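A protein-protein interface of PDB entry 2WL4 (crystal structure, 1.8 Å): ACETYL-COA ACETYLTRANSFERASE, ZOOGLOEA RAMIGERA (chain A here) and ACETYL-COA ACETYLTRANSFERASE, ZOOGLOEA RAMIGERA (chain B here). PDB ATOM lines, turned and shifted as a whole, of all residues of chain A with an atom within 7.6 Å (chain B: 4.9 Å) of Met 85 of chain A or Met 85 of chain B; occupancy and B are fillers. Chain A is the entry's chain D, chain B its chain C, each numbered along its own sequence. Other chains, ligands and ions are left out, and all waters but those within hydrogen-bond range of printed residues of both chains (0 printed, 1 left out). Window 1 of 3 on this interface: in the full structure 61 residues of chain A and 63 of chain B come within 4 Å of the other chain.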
ATOM      1  N   ILE A  53      23.322  19.323  15.294  1.00  0.00           N
ATOM      2  CA  ILE A  53      23.930  20.513  14.707  1.00  0.00           C
ATOM      3  C   ILE A  53      25.249  20.858  15.405  1.00  0.00           C
ATOM      4  O   ILE A  53      25.266  21.227  16.581  1.00  0.00           O
ATOM      5  CB  ILE A  53      22.979  21.718  14.803  1.00  0.00           C
ATOM      6  CG1 ILE A  53      21.562  21.316  14.384  1.00  0.00           C
ATOM      7  CG2 ILE A  53      23.483  22.869  13.950  1.00  0.00           C
ATOM      8  CD1 ILE A  53      20.557  22.455  14.452  1.00  0.00           C
ATOM      9  N   LEU A  54      26.360  20.728  14.685  1.00  0.00           N
ATOM     10  CA  LEU A  54      27.659  20.969  15.289  1.00  0.00           C
ATOM     11  C   LEU A  54      28.489  21.958  14.490  1.00  0.00           C
ATOM     12  O   LEU A  54      28.777  21.733  13.312  1.00  0.00           O
ATOM     13  CB  LEU A  54      28.433  19.650  15.411  1.00  0.00           C
ATOM     14  CG  LEU A  54      27.843  18.597  16.351  1.00  0.00           C
ATOM     15  CD1 LEU A  54      28.332  17.197  15.983  1.00  0.00           C
ATOM     16  CD2 LEU A  54      28.178  18.930  17.798  1.00  0.00           C
ATOM     17  N   GLY A  55      28.905  23.046  15.129  1.00  0.00           N
ATOM     18  CA  GLY A  55      29.814  23.969  14.463  1.00  0.00           C
ATOM     19  C   GLY A  55      31.203  23.396  14.226  1.00  0.00           C
ATOM     20  O   GLY A  55      31.741  22.679  15.071  1.00  0.00           O
ATOM     21  N   GLN A  56      31.788  23.706  13.071  1.00  0.00           N
ATOM     22  CA  GLN A  56      33.132  23.241  12.734  1.00  0.00           C
ATOM     23  C   GLN A  56      33.709  24.092  11.615  1.00  0.00           C
ATOM     24  O   GLN A  56      33.119  24.185  10.541  1.00  0.00           O
ATOM     25  CB  GLN A  56      33.107  21.761  12.325  1.00  0.00           C
ATOM     26  CG  GLN A  56      34.489  21.153  12.117  1.00  0.00           C
ATOM     27  CD  GLN A  56      34.448  19.680  11.701  1.00  0.00           C
ATOM     28  OE1 GLN A  56      33.378  19.105  11.491  1.00  0.00           O
ATOM     29  NE2 GLN A  56      35.623  19.068  11.587  1.00  0.00           N
ATOM     30  N   VAL A  57      34.865  24.704  11.859  1.00  0.00           N
ATOM     31  CA  VAL A  57      35.501  25.574  10.865  1.00  0.00           C
ATOM     32  C   VAL A  57      36.554  24.882   9.965  1.00  0.00           C
ATOM     33  O   VAL A  57      36.730  25.272   8.806  1.00  0.00           O
ATOM     34  CB  VAL A  57      36.133  26.821  11.543  1.00  0.00           C
ATOM     35  CG1 VAL A  57      36.618  27.820  10.493  1.00  0.00           C
ATOM     36  CG2 VAL A  57      35.136  27.483  12.487  1.00  0.00           C
ATOM     37  N   LEU A  58      37.239  23.863  10.487  1.00  0.00           N
ATOM     38  CA  LEU A  58      38.339  23.218   9.754  1.00  0.00           C
ATOM     39  C   LEU A  58      38.128  21.733   9.413  1.00  0.00           C
ATOM     40  O   LEU A  58      38.904  20.878   9.856  1.00  0.00           O
ATOM     41  CB  LEU A  58      39.638  23.343  10.558  1.00  0.00           C
ATOM     42  CG  LEU A  58      39.950  24.717  11.136  1.00  0.00           C
ATOM     43  CD1 LEU A  58      41.207  24.667  12.000  1.00  0.00           C
ATOM     44  CD2 LEU A  58      40.059  25.760  10.026  1.00  0.00           C
ATOM     45  N   PRO A  59      37.108  21.423   8.596  1.00  0.00           N
ATOM     46  CA  PRO A  59      36.763  20.032   8.280  1.00  0.00           C
ATOM     47  C   PRO A  59      37.476  19.439   7.051  1.00  0.00           C
ATOM     48  O   PRO A  59      37.239  18.275   6.726  1.00  0.00           O
ATOM     49  CB  PRO A  59      35.250  20.107   8.004  1.00  0.00           C
ATOM     50  CG  PRO A  59      34.836  21.538   8.311  1.00  0.00           C
ATOM     51  CD  PRO A  59      36.067  22.346   8.122  1.00  0.00           C
ATOM     52  N   ASN A  65      30.440  15.682   5.441  1.00  0.00           N
ATOM     53  CA  ASN A  65      29.604  16.104   6.561  1.00  0.00           C
ATOM     54  C   ASN A  65      29.947  15.384   7.866  1.00  0.00           C
ATOM     55  O   ASN A  65      29.274  14.425   8.244  1.00  0.00           O
ATOM     56  CB  ASN A  65      28.138  15.868   6.195  1.00  0.00           C
ATOM     57  CG  ASN A  65      27.179  16.358   7.254  1.00  0.00           C
ATOM     58  OD1 ASN A  65      27.512  17.225   8.065  1.00  0.00           O
ATOM     59  ND2 ASN A  65      25.971  15.805   7.249  1.00  0.00           N
ATOM     60  N   ALA A  67      29.572  16.155  10.864  1.00  0.00           N
ATOM     61  CA  ALA A  67      28.534  16.266  11.879  1.00  0.00           C
ATOM     62  C   ALA A  67      27.669  15.009  11.891  1.00  0.00           C
ATOM     63  O   ALA A  67      27.150  14.603  12.938  1.00  0.00           O
ATOM     64  CB  ALA A  67      27.668  17.516  11.633  1.00  0.00           C
ATOM     65  N   TRP A  83      23.830  18.270  10.449  1.00  0.00           N
ATOM     66  CA  TRP A  83      24.577  19.143   9.553  1.00  0.00           C
ATOM     67  C   TRP A  83      25.586  19.984  10.322  1.00  0.00           C
ATOM     68  O   TRP A  83      25.444  20.194  11.529  1.00  0.00           O
ATOM     69  CB  TRP A  83      23.626  20.051   8.776  1.00  0.00           C
ATOM     70  CG  TRP A  83      22.634  20.770   9.640  1.00  0.00           C
ATOM     71  CD1 TRP A  83      21.473  20.263  10.151  1.00  0.00           C
ATOM     72  CD2 TRP A  83      22.706  22.131  10.080  1.00  0.00           C
ATOM     73  NE1 TRP A  83      20.820  21.224  10.886  1.00  0.00           N
ATOM     74  CE2 TRP A  83      21.556  22.382  10.858  1.00  0.00           C
ATOM     75  CE3 TRP A  83      23.629  23.165   9.893  1.00  0.00           C
ATOM     76  CZ2 TRP A  83      21.306  23.620  11.447  1.00  0.00           C
ATOM     77  CZ3 TRP A  83      23.380  24.394  10.480  1.00  0.00           C
ATOM     78  CH2 TRP A  83      22.229  24.611  11.248  1.00  0.00           C
ATOM     79  N   GLY A  84      26.599  20.468   9.611  1.00  0.00           N
ATOM     80  CA  GLY A  84      27.604  21.338  10.189  1.00  0.00           C
ATOM     81  C   GLY A  84      27.444  22.767   9.711  1.00  0.00           C
ATOM     82  O   GLY A  84      26.846  23.024   8.670  1.00  0.00           O
ATOM     83  N   MET A  85      27.977  23.708  10.476  1.00  0.00           N
ATOM     84  CA  MET A  85      27.875  25.113  10.104  1.00  0.00           C
ATOM     85  C   MET A  85      29.095  25.889  10.583  1.00  0.00           C
ATOM     86  O   MET A  85      29.902  25.380  11.349  1.00  0.00           O
ATOM     87  CB  MET A  85      26.568  25.730  10.621  1.00  0.00           C
ATOM     88  CG  MET A  85      26.247  25.460  12.087  1.00  0.00           C
ATOM     89  SD  MET A  85      27.036  26.623  13.217  1.00  0.00           S
ATOM     90  CE  MET A  85      26.545  28.171  12.470  1.00  0.00           C
ATOM     91  N   ASN A  86      29.212  27.130  10.135  1.00  0.00           N
ATOM     92  CA  ASN A  86      30.403  27.917  10.392  1.00  0.00           C
ATOM     93  C   ASN A  86      30.058  29.379  10.635  1.00  0.00           C
ATOM     94  O   ASN A  86      29.630  30.072   9.723  1.00  0.00           O
ATOM     95  CB  ASN A  86      31.350  27.783   9.186  1.00  0.00           C
ATOM     96  CG  ASN A  86      32.709  28.444   9.404  1.00  0.00           C
ATOM     97  OD1 ASN A  86      32.891  29.244  10.313  1.00  0.00           O
ATOM     98  ND2 ASN A  86      33.668  28.099   8.559  1.00  0.00           N
ATOM     99  N   GLN A  87      30.216  29.837  11.870  1.00  0.00           N
ATOM    100  CA  GLN A  87      30.264  31.271  12.137  1.00  0.00           C
ATOM    101  C   GLN A  87      31.523  31.564  12.938  1.00  0.00           C
ATOM    102  O   GLN A  87      31.500  32.280  13.944  1.00  0.00           O
ATOM    103  CB  GLN A  87      29.026  31.764  12.870  1.00  0.00           C
ATOM    104  CG  GLN A  87      28.874  33.268  12.807  1.00  0.00           C
ATOM    105  CD  GLN A  87      27.474  33.711  13.136  1.00  0.00           C
ATOM    106  OE1 GLN A  87      26.667  32.930  13.641  1.00  0.00           O
ATOM    107  NE2 GLN A  87      27.174  34.975  12.859  1.00  0.00           N
ATOM    108  N   LEU A  88      32.620  30.979  12.465  1.00  0.00           N
ATOM    109  CA  LEU A  88      33.930  31.106  13.095  1.00  0.00           C
ATOM    110  C   LEU A  88      33.912  30.900  14.597  1.00  0.00           C
ATOM    111  O   LEU A  88      33.476  29.855  15.073  1.00  0.00           O
ATOM    112  CB  LEU A  88      34.584  32.438  12.733  1.00  0.00           C
ATOM    113  CG  LEU A  88      35.019  32.421  11.270  1.00  0.00           C
ATOM    114  CD1 LEU A  88      35.622  33.749  10.863  1.00  0.00           C
ATOM    115  CD2 LEU A  88      35.979  31.249  11.010  1.00  0.00           C
ATOM    116  N   GLY A  90      32.159  31.793  16.811  1.00  0.00           N
ATOM    117  CA  GLY A  90      30.847  31.701  17.420  1.00  0.00           C
ATOM    118  C   GLY A  90      30.027  30.576  16.826  1.00  0.00           C
ATOM    119  O   GLY A  90      28.797  30.618  16.839  1.00  0.00           O
ATOM    120  N   SER A  91      30.703  29.560  16.307  1.00  0.00           N
ATOM    121  CA  SER A  91      30.018  28.438  15.681  1.00  0.00           C
ATOM    122  C   SER A  91      29.284  27.607  16.734  1.00  0.00           C
ATOM    123  O   SER A  91      28.102  27.290  16.575  1.00  0.00           O
ATOM    124  CB  SER A  91      31.012  27.574  14.901  1.00  0.00           C
ATOM    125  OG  SER A  91      31.629  28.318  13.859  1.00  0.00           O
ATOM    126  N   GLY A  92      29.996  27.274  17.811  1.00  0.00           N
ATOM    127  CA  GLY A  92      29.475  26.438  18.884  1.00  0.00           C
ATOM    128  C   GLY A  92      28.359  26.998  19.753  1.00  0.00           C
ATOM    129  O   GLY A  92      27.645  26.231  20.404  1.00  0.00           O
ATOM    130  N   LEU A  93      28.219  28.322  19.803  1.00  0.00           N
ATOM    131  CA  LEU A  93      27.120  28.946  20.539  1.00  0.00           C
ATOM    132  C   LEU A  93      25.968  29.294  19.602  1.00  0.00           C
ATOM    133  O   LEU A  93      24.793  29.206  19.980  1.00  0.00           O
ATOM    134  CB  LEU A  93      27.591  30.204  21.276  1.00  0.00           C
ATOM    135  CG  LEU A  93      26.482  31.084  21.854  1.00  0.00           C
ATOM    136  CD1 LEU A  93      25.867  30.462  23.108  1.00  0.00           C
ATOM    137  CD2 LEU A  93      27.016  32.478  22.148  1.00  0.00           C
ATOM    138  N   ARG A  94      26.311  29.697  18.379  1.00  0.00           N
ATOM    139  CA  ARG A  94      25.291  30.007  17.385  1.00  0.00           C
ATOM    140  C   ARG A  94      24.547  28.731  17.024  1.00  0.00           C
ATOM    141  O   ARG A  94      23.336  28.758  16.769  1.00  0.00           O
ATOM    142  CB  ARG A  94      25.898  30.661  16.145  1.00  0.00           C
ATOM    143  CG  ARG A  94      24.894  30.918  15.029  1.00  0.00           C
ATOM    144  CD  ARG A  94      23.632  31.637  15.506  1.00  0.00           C
ATOM    145  NE  ARG A  94      22.610  31.603  14.464  1.00  0.00           N
ATOM    146  CZ  ARG A  94      22.657  32.331  13.351  1.00  0.00           C
ATOM    147  NH1 ARG A  94      23.677  33.154  13.134  1.00  0.00           N
ATOM    148  NH2 ARG A  94      21.691  32.232  12.450  1.00  0.00           N
ATOM    149  N   ALA A  95      25.276  27.615  17.031  1.00  0.00           N
ATOM    150  CA  ALA A  95      24.664  26.298  16.914  1.00  0.00           C
ATOM    151  C   ALA A  95      23.534  26.153  17.932  1.00  0.00           C
ATOM    152  O   ALA A  95      22.407  25.810  17.580  1.00  0.00           O
ATOM    153  CB  ALA A  95      25.694  25.199  17.134  1.00  0.00           C
ATOM    154  N   VAL A  96      23.845  26.419  19.198  1.00  0.00           N
ATOM    155  CA  VAL A  96      22.876  26.229  20.278  1.00  0.00           C
ATOM    156  C   VAL A  96      21.541  26.901  19.973  1.00  0.00           C
ATOM    157  O   VAL A  96      20.473  26.315  20.179  1.00  0.00           O
ATOM    158  CB  VAL A  96      23.403  26.753  21.627  1.00  0.00           C
ATOM    159  CG1 VAL A  96      22.303  26.692  22.681  1.00  0.00           C
ATOM    160  CG2 VAL A  96      24.613  25.944  22.062  1.00  0.00           C
ATOM    161  N   LEU A  98      20.502  27.925  16.958  1.00  0.00           N
ATOM    162  CA  LEU A  98      20.005  27.236  15.768  1.00  0.00           C
ATOM    163  C   LEU A  98      19.371  25.920  16.200  1.00  0.00           C
ATOM    164  O   LEU A  98      18.375  25.473  15.628  1.00  0.00           O
ATOM    165  CB  LEU A  98      21.145  26.971  14.770  1.00  0.00           C
ATOM    166  CG  LEU A  98      21.745  28.172  14.032  1.00  0.00           C
ATOM    167  CD1 LEU A  98      22.973  27.731  13.255  1.00  0.00           C
ATOM    168  CD2 LEU A  98      20.739  28.832  13.088  1.00  0.00           C
ATOM    169  N   GLY A 114      26.065  21.774  19.240  1.00  0.00           N
ATOM    170  CA  GLY A 114      27.355  22.114  19.809  1.00  0.00           C
ATOM    171  C   GLY A 114      28.403  22.528  18.797  1.00  0.00           C
ATOM    172  O   GLY A 114      28.113  23.226  17.823  1.00  0.00           O
ATOM    173  N   GLY A 115      29.635  22.086  19.036  1.00  0.00           N
ATOM    174  CA  GLY A 115      30.757  22.457  18.207  1.00  0.00           C
ATOM    175  C   GLY A 115      31.892  21.471  18.398  1.00  0.00           C
ATOM    176  O   GLY A 115      32.057  20.902  19.481  1.00  0.00           O
ATOM    177  N   MET A 116      32.661  21.257  17.337  1.00  0.00           N
ATOM    178  CA  MET A 116      33.799  20.356  17.386  1.00  0.00           C
ATOM    179  C   MET A 116      34.913  20.892  16.496  1.00  0.00           C
ATOM    180  O   MET A 116      34.655  21.447  15.423  1.00  0.00           O
ATOM    181  CB  MET A 116      33.395  18.943  16.960  1.00  0.00           C
ATOM    182  CG  MET A 116      32.904  18.821  15.525  1.00  0.00           C
ATOM    183  SD  MET A 116      32.787  17.089  15.041  1.00  0.00           S
ATOM    184  CE  MET A 116      32.096  17.226  13.383  1.00  0.00           C
ATOM    185  N   GLU A 117      36.151  20.742  16.957  1.00  0.00           N
ATOM    186  CA  GLU A 117      37.286  21.232  16.198  1.00  0.00           C
ATOM    187  C   GLU A 117      38.580  20.551  16.585  1.00  0.00           C
ATOM    188  O   GLU A 117      38.927  20.478  17.763  1.00  0.00           O
ATOM    189  CB  GLU A 117      37.442  22.743  16.367  1.00  0.00           C
ATOM    190  CG  GLU A 117      38.259  23.383  15.274  1.00  0.00           C
ATOM    191  CD  GLU A 117      37.433  23.738  14.052  1.00  0.00           C
ATOM    192  OE1 GLU A 117      37.610  23.082  12.999  1.00  0.00           O
ATOM    193  OE2 GLU A 117      36.616  24.684  14.140  1.00  0.00           O
ATOM    194  N   GLY A 351      35.579  26.083  16.290  1.00  0.00           N
ATOM    195  CA  GLY A 351      34.214  25.608  16.145  1.00  0.00           C
ATOM    196  C   GLY A 351      33.535  25.060  17.388  1.00  0.00           C
ATOM    197  O   GLY A 351      32.311  24.961  17.437  1.00  0.00           O
ATOM    198  N   ILE B  53      22.853  33.734   4.967  1.00  0.00           N
ATOM    199  CA  ILE B  53      23.076  32.320   5.249  1.00  0.00           C
ATOM    200  C   ILE B  53      23.300  31.494   3.979  1.00  0.00           C
ATOM    201  O   ILE B  53      22.358  31.192   3.245  1.00  0.00           O
ATOM    202  CB  ILE B  53      21.902  31.732   6.048  1.00  0.00           C
ATOM    203  CG1 ILE B  53      21.749  32.474   7.377  1.00  0.00           C
ATOM    204  CG2 ILE B  53      22.103  30.247   6.279  1.00  0.00           C
ATOM    205  CD1 ILE B  53      20.327  32.542   7.879  1.00  0.00           C
ATOM    206  N   LEU B  54      24.551  31.119   3.731  1.00  0.00           N
ATOM    207  CA  LEU B  54      24.905  30.416   2.504  1.00  0.00           C
ATOM    208  C   LEU B  54      25.413  28.981   2.717  1.00  0.00           C
ATOM    209  O   LEU B  54      26.323  28.736   3.503  1.00  0.00           O
ATOM    210  CB  LEU B  54      25.937  31.230   1.713  1.00  0.00           C
ATOM    211  CG  LEU B  54      25.360  32.379   0.885  1.00  0.00           C
ATOM    212  CD1 LEU B  54      26.461  33.280   0.347  1.00  0.00           C
ATOM    213  CD2 LEU B  54      24.488  31.836  -0.246  1.00  0.00           C
ATOM    214  N   GLY B  55      24.811  28.034   2.005  1.00  0.00           N
ATOM    215  CA  GLY B  55      25.289  26.667   2.018  1.00  0.00           C
ATOM    216  C   GLY B  55      26.574  26.536   1.220  1.00  0.00           C
ATOM    217  O   GLY B  55      26.658  27.017   0.087  1.00  0.00           O
ATOM    218  N   GLN B  56      27.578  25.894   1.811  1.00  0.00           N
ATOM    219  CA  GLN B  56      28.841  25.665   1.125  1.00  0.00           C
ATOM    220  C   GLN B  56      29.486  24.390   1.644  1.00  0.00           C
ATOM    221  O   GLN B  56      29.540  24.166   2.852  1.00  0.00           O
ATOM    222  CB  GLN B  56      29.797  26.852   1.312  1.00  0.00           C
ATOM    223  CG  GLN B  56      31.090  26.734   0.521  1.00  0.00           C
ATOM    224  CD  GLN B  56      31.894  28.023   0.528  1.00  0.00           C
ATOM    225  OE1 GLN B  56      31.707  28.883   1.393  1.00  0.00           O
ATOM    226  NE2 GLN B  56      32.798  28.162  -0.436  1.00  0.00           N
ATOM    227  N   TRP B  83      26.905  33.654   7.900  1.00  0.00           N
ATOM    228  CA  TRP B  83      27.495  32.351   8.180  1.00  0.00           C
ATOM    229  C   TRP B  83      27.194  31.336   7.083  1.00  0.00           C
ATOM    230  O   TRP B  83      26.337  31.561   6.228  1.00  0.00           O
ATOM    231  CB  TRP B  83      27.028  31.814   9.539  1.00  0.00           C
ATOM    232  CG  TRP B  83      25.545  31.868   9.745  1.00  0.00           C
ATOM    233  CD1 TRP B  83      24.794  32.982   9.963  1.00  0.00           C
ATOM    234  CD2 TRP B  83      24.632  30.759   9.767  1.00  0.00           C
ATOM    235  NE1 TRP B  83      23.471  32.643  10.114  1.00  0.00           N
ATOM    236  CE2 TRP B  83      23.346  31.282   9.998  1.00  0.00           C
ATOM    237  CE3 TRP B  83      24.777  29.376   9.608  1.00  0.00           C
ATOM    238  CZ2 TRP B  83      22.210  30.474  10.080  1.00  0.00           C
ATOM    239  CZ3 TRP B  83      23.645  28.568   9.696  1.00  0.00           C
ATOM    240  CH2 TRP B  83      22.378  29.126   9.925  1.00  0.00           C
ATOM    241  N   GLY B  84      27.911  30.218   7.114  1.00  0.00           N
ATOM    242  CA  GLY B  84      27.718  29.148   6.156  1.00  0.00           C
ATOM    243  C   GLY B  84      27.328  27.846   6.827  1.00  0.00           C
ATOM    244  O   GLY B  84      27.578  27.651   8.017  1.00  0.00           O
ATOM    245  N   MET B  85      26.716  26.948   6.060  1.00  0.00           N
ATOM    246  CA  MET B  85      26.306  25.648   6.576  1.00  0.00           C
ATOM    247  C   MET B  85      26.554  24.552   5.543  1.00  0.00           C
ATOM    248  O   MET B  85      26.913  24.839   4.395  1.00  0.00           O
ATOM    249  CB  MET B  85      24.838  25.680   7.018  1.00  0.00           C
ATOM    250  CG  MET B  85      23.886  26.308   6.006  1.00  0.00           C
ATOM    251  SD  MET B  85      23.355  25.126   4.758  1.00  0.00           S
ATOM    252  CE  MET B  85      22.714  23.810   5.785  1.00  0.00           C
ATOM    253  N   ASN B  86      26.350  23.305   5.955  1.00  0.00           N
ATOM    254  CA  ASN B  86      26.736  22.139   5.166  1.00  0.00           C
ATOM    255  C   ASN B  86      25.893  20.894   5.422  1.00  0.00           C
ATOM    256  O   ASN B  86      26.283  20.019   6.195  1.00  0.00           O
ATOM    257  CB  ASN B  86      28.205  21.789   5.439  1.00  0.00           C
ATOM    258  CG  ASN B  86      28.655  20.525   4.719  1.00  0.00           C
ATOM    259  OD1 ASN B  86      27.931  19.982   3.883  1.00  0.00           O
ATOM    260  ND2 ASN B  86      29.864  20.057   5.036  1.00  0.00           N
ATOM    261  N   GLN B  87      24.741  20.814   4.777  1.00  0.00           N
ATOM    262  CA  GLN B  87      24.019  19.555   4.704  1.00  0.00           C
ATOM    263  C   GLN B  87      24.246  19.021   3.297  1.00  0.00           C
ATOM    264  O   GLN B  87      23.354  18.437   2.675  1.00  0.00           O
ATOM    265  CB  GLN B  87      22.529  19.742   4.997  1.00  0.00           C
ATOM    266  CG  GLN B  87      21.782  18.425   5.177  1.00  0.00           C
ATOM    267  CD  GLN B  87      20.398  18.601   5.771  1.00  0.00           C
ATOM    268  OE1 GLN B  87      19.895  19.719   5.887  1.00  0.00           O
ATOM    269  NE2 GLN B  87      19.773  17.490   6.150  1.00  0.00           N
ATOM    270  N   SER B  91      22.282  21.562   1.555  1.00  0.00           N
ATOM    271  CA  SER B  91      22.634  22.835   2.176  1.00  0.00           C
ATOM    272  C   SER B  91      21.907  24.026   1.558  1.00  0.00           C
ATOM    273  O   SER B  91      21.325  24.840   2.273  1.00  0.00           O
ATOM    274  CB  SER B  91      24.147  23.047   2.119  1.00  0.00           C
ATOM    275  OG  SER B  91      24.820  21.935   2.686  1.00  0.00           O
ATOM    276  N   GLY B  92      21.947  24.116   0.231  1.00  0.00           N
ATOM    277  CA  GLY B  92      21.324  25.210  -0.499  1.00  0.00           C
ATOM    278  C   GLY B  92      19.869  25.492  -0.174  1.00  0.00           C
ATOM    279  O   GLY B  92      19.443  26.651  -0.225  1.00  0.00           O
ATOM    280  N   ARG B  94      18.237  23.885   2.782  1.00  0.00           N
ATOM    281  CA  ARG B  94      18.174  23.983   4.234  1.00  0.00           C
ATOM    282  C   ARG B  94      18.476  25.428   4.633  1.00  0.00           C
ATOM    283  O   ARG B  94      17.917  25.948   5.598  1.00  0.00           O
ATOM    284  CB  ARG B  94      19.149  23.011   4.908  1.00  0.00           C
ATOM    285  CG  ARG B  94      18.974  22.905   6.424  1.00  0.00           C
ATOM    286  CD  ARG B  94      17.576  22.431   6.799  1.00  0.00           C
ATOM    287  NE  ARG B  94      17.357  22.416   8.244  1.00  0.00           N
ATOM    288  CZ  ARG B  94      17.703  21.411   9.039  1.00  0.00           C
ATOM    289  NH1 ARG B  94      18.292  20.334   8.531  1.00  0.00           N
ATOM    290  NH2 ARG B  94      17.464  21.481  10.341  1.00  0.00           N
ATOM    291  N   ALA B  95      19.343  26.073   3.856  1.00  0.00           N
ATOM    292  CA  ALA B  95      19.740  27.456   4.104  1.00  0.00           C
ATOM    293  C   ALA B  95      18.543  28.402   4.097  1.00  0.00           C
ATOM    294  O   ALA B  95      18.327  29.153   5.053  1.00  0.00           O
ATOM    295  CB  ALA B  95      20.783  27.900   3.081  1.00  0.00           C
ATOM    296  N   LEU B  98      16.570  27.600   7.121  1.00  0.00           N
ATOM    297  CA  LEU B  98      17.209  28.208   8.280  1.00  0.00           C
ATOM    298  C   LEU B  98      16.839  29.685   8.326  1.00  0.00           C
ATOM    299  O   LEU B  98      16.543  30.232   9.391  1.00  0.00           O
ATOM    300  CB  LEU B  98      18.727  28.029   8.223  1.00  0.00           C
ATOM    301  CG  LEU B  98      19.195  26.641   8.651  1.00  0.00           C
ATOM    302  CD1 LEU B  98      20.709  26.576   8.712  1.00  0.00           C
ATOM    303  CD2 LEU B  98      18.583  26.288   9.997  1.00  0.00           C
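O of Gly 84 of chain B sits at hydrogen-bond distance from N of Asn 86 of chain A, at 2.7 Å. The backbone carbonyl oxygen (O) of Gly 84 of chain A is in hydrogen-bond range of the backbone NH (N) of Asn 86 of chain B. The guanidinium group (NH2) of Arg 94 of chain B lies close to the indole nitrogen (NE1) of Trp 83 of chain A (3.4 Å). NH2 of Arg 94 of chain A lies close to NE1 of Trp 83 of chain B, at 3.0 Å.
The backbone NH (N) of Met 85 of chain B sits at hydrogen-bond distance from the backbone carbonyl oxygen (O) of Leu 54 of chain B (3.1 Å). The backbone carbonyl oxygen of Met 85 of chain B sits at hydrogen-bond distance from the backbone NH of Gln 56 of chain B (2.9 Å). NH1 of Arg 94 of chain B lies within hydrogen-bond range of OE1 of Gln 87 of chain B. The backbone carbonyl oxygen (O) of Trp 83 of chain A is in hydrogen-bond range of the backbone NH (N) of Leu 54 of chain A. N of Gln 56 of chain A sits at hydrogen-bond distance from O of Met 85 of chain A (3.1 Å). N of Gln 87 of chain A sits at hydrogen-bond distance from OG of Ser 91 of chain A, 2.9 Å away.
Among the printed residues, pairs that only touch across the chains: Asn 86 of chain A with Trp 83 of chain B (3.1 Å), Met 85 of chain A with Gly 84 of chain B (3.3 Å), Gly 84 of chain A with Met 85 of chain B (3.4 Å), Trp 83 of chain A with Leu 98 of chain B (3.6 Å), Met 85 of chain A with Trp 83 of chain B (3.6 Å), Leu 98 of chain A with Trp 83 of chain B (3.6 Å), Asn 65 of chain A with Asn 86 of chain B (3.6 Å), Trp 83 of chain A with Asn 86 of chain B (3.7 Å), Gln 87 of chain A with Trp 83 of chain B (3.9 Å), Met 85 of chain A with Met 85 of chain B (3.9 Å), Trp 83 of chain A with Gln 87 of chain B (3.9 Å) and Trp 83 of chain A with Met 85 of chain B (3.97 Å).
Met 85 of chain A touches just these residues of chain B: Trp 83, Gly 84 and Met 85. Met 85 of chain B touches three residues of chain A. Of the printed residues of chain B, Gly 84 of chain A touches Met 85 (3.4 Å) and Asn 86 (2.8 Å). Printed residues of chain A within 4 Å of Arg 94 of chain B: Trp 83. Of the printed residues of chain A, Asn 86 of chain B touches Asn 65 (3.6 Å), Trp 83 (3.7 Å) and Gly 84 (2.8 Å). Of the printed residues of chain B, Gln 87 of chain A touches Trp 83 (3.9 Å). Of the printed residues of chain B, Arg 94 of chain A touches Trp 83. Ile 53 of chain B touches none of the printed residues of chain A. The nearest residue of chain B that does not touch Met 85 of chain A is Asn 86 of chain B (4.8 Å).
Printed residues of chain B that touch a printed residue of chain A: Trp 83, Gly 84, Met 85, Asn 86, Gln 87, Arg 94 and Leu 98. Hydrophobic or aromatic side chains of chain B that line the printed part of chain A: Trp 83, Met 85 and Leu 98. Of the 28 printed residues of chain A, 8 touch a printed residue of chain B. Among the printed residues, 16 pairs touch across the chains.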
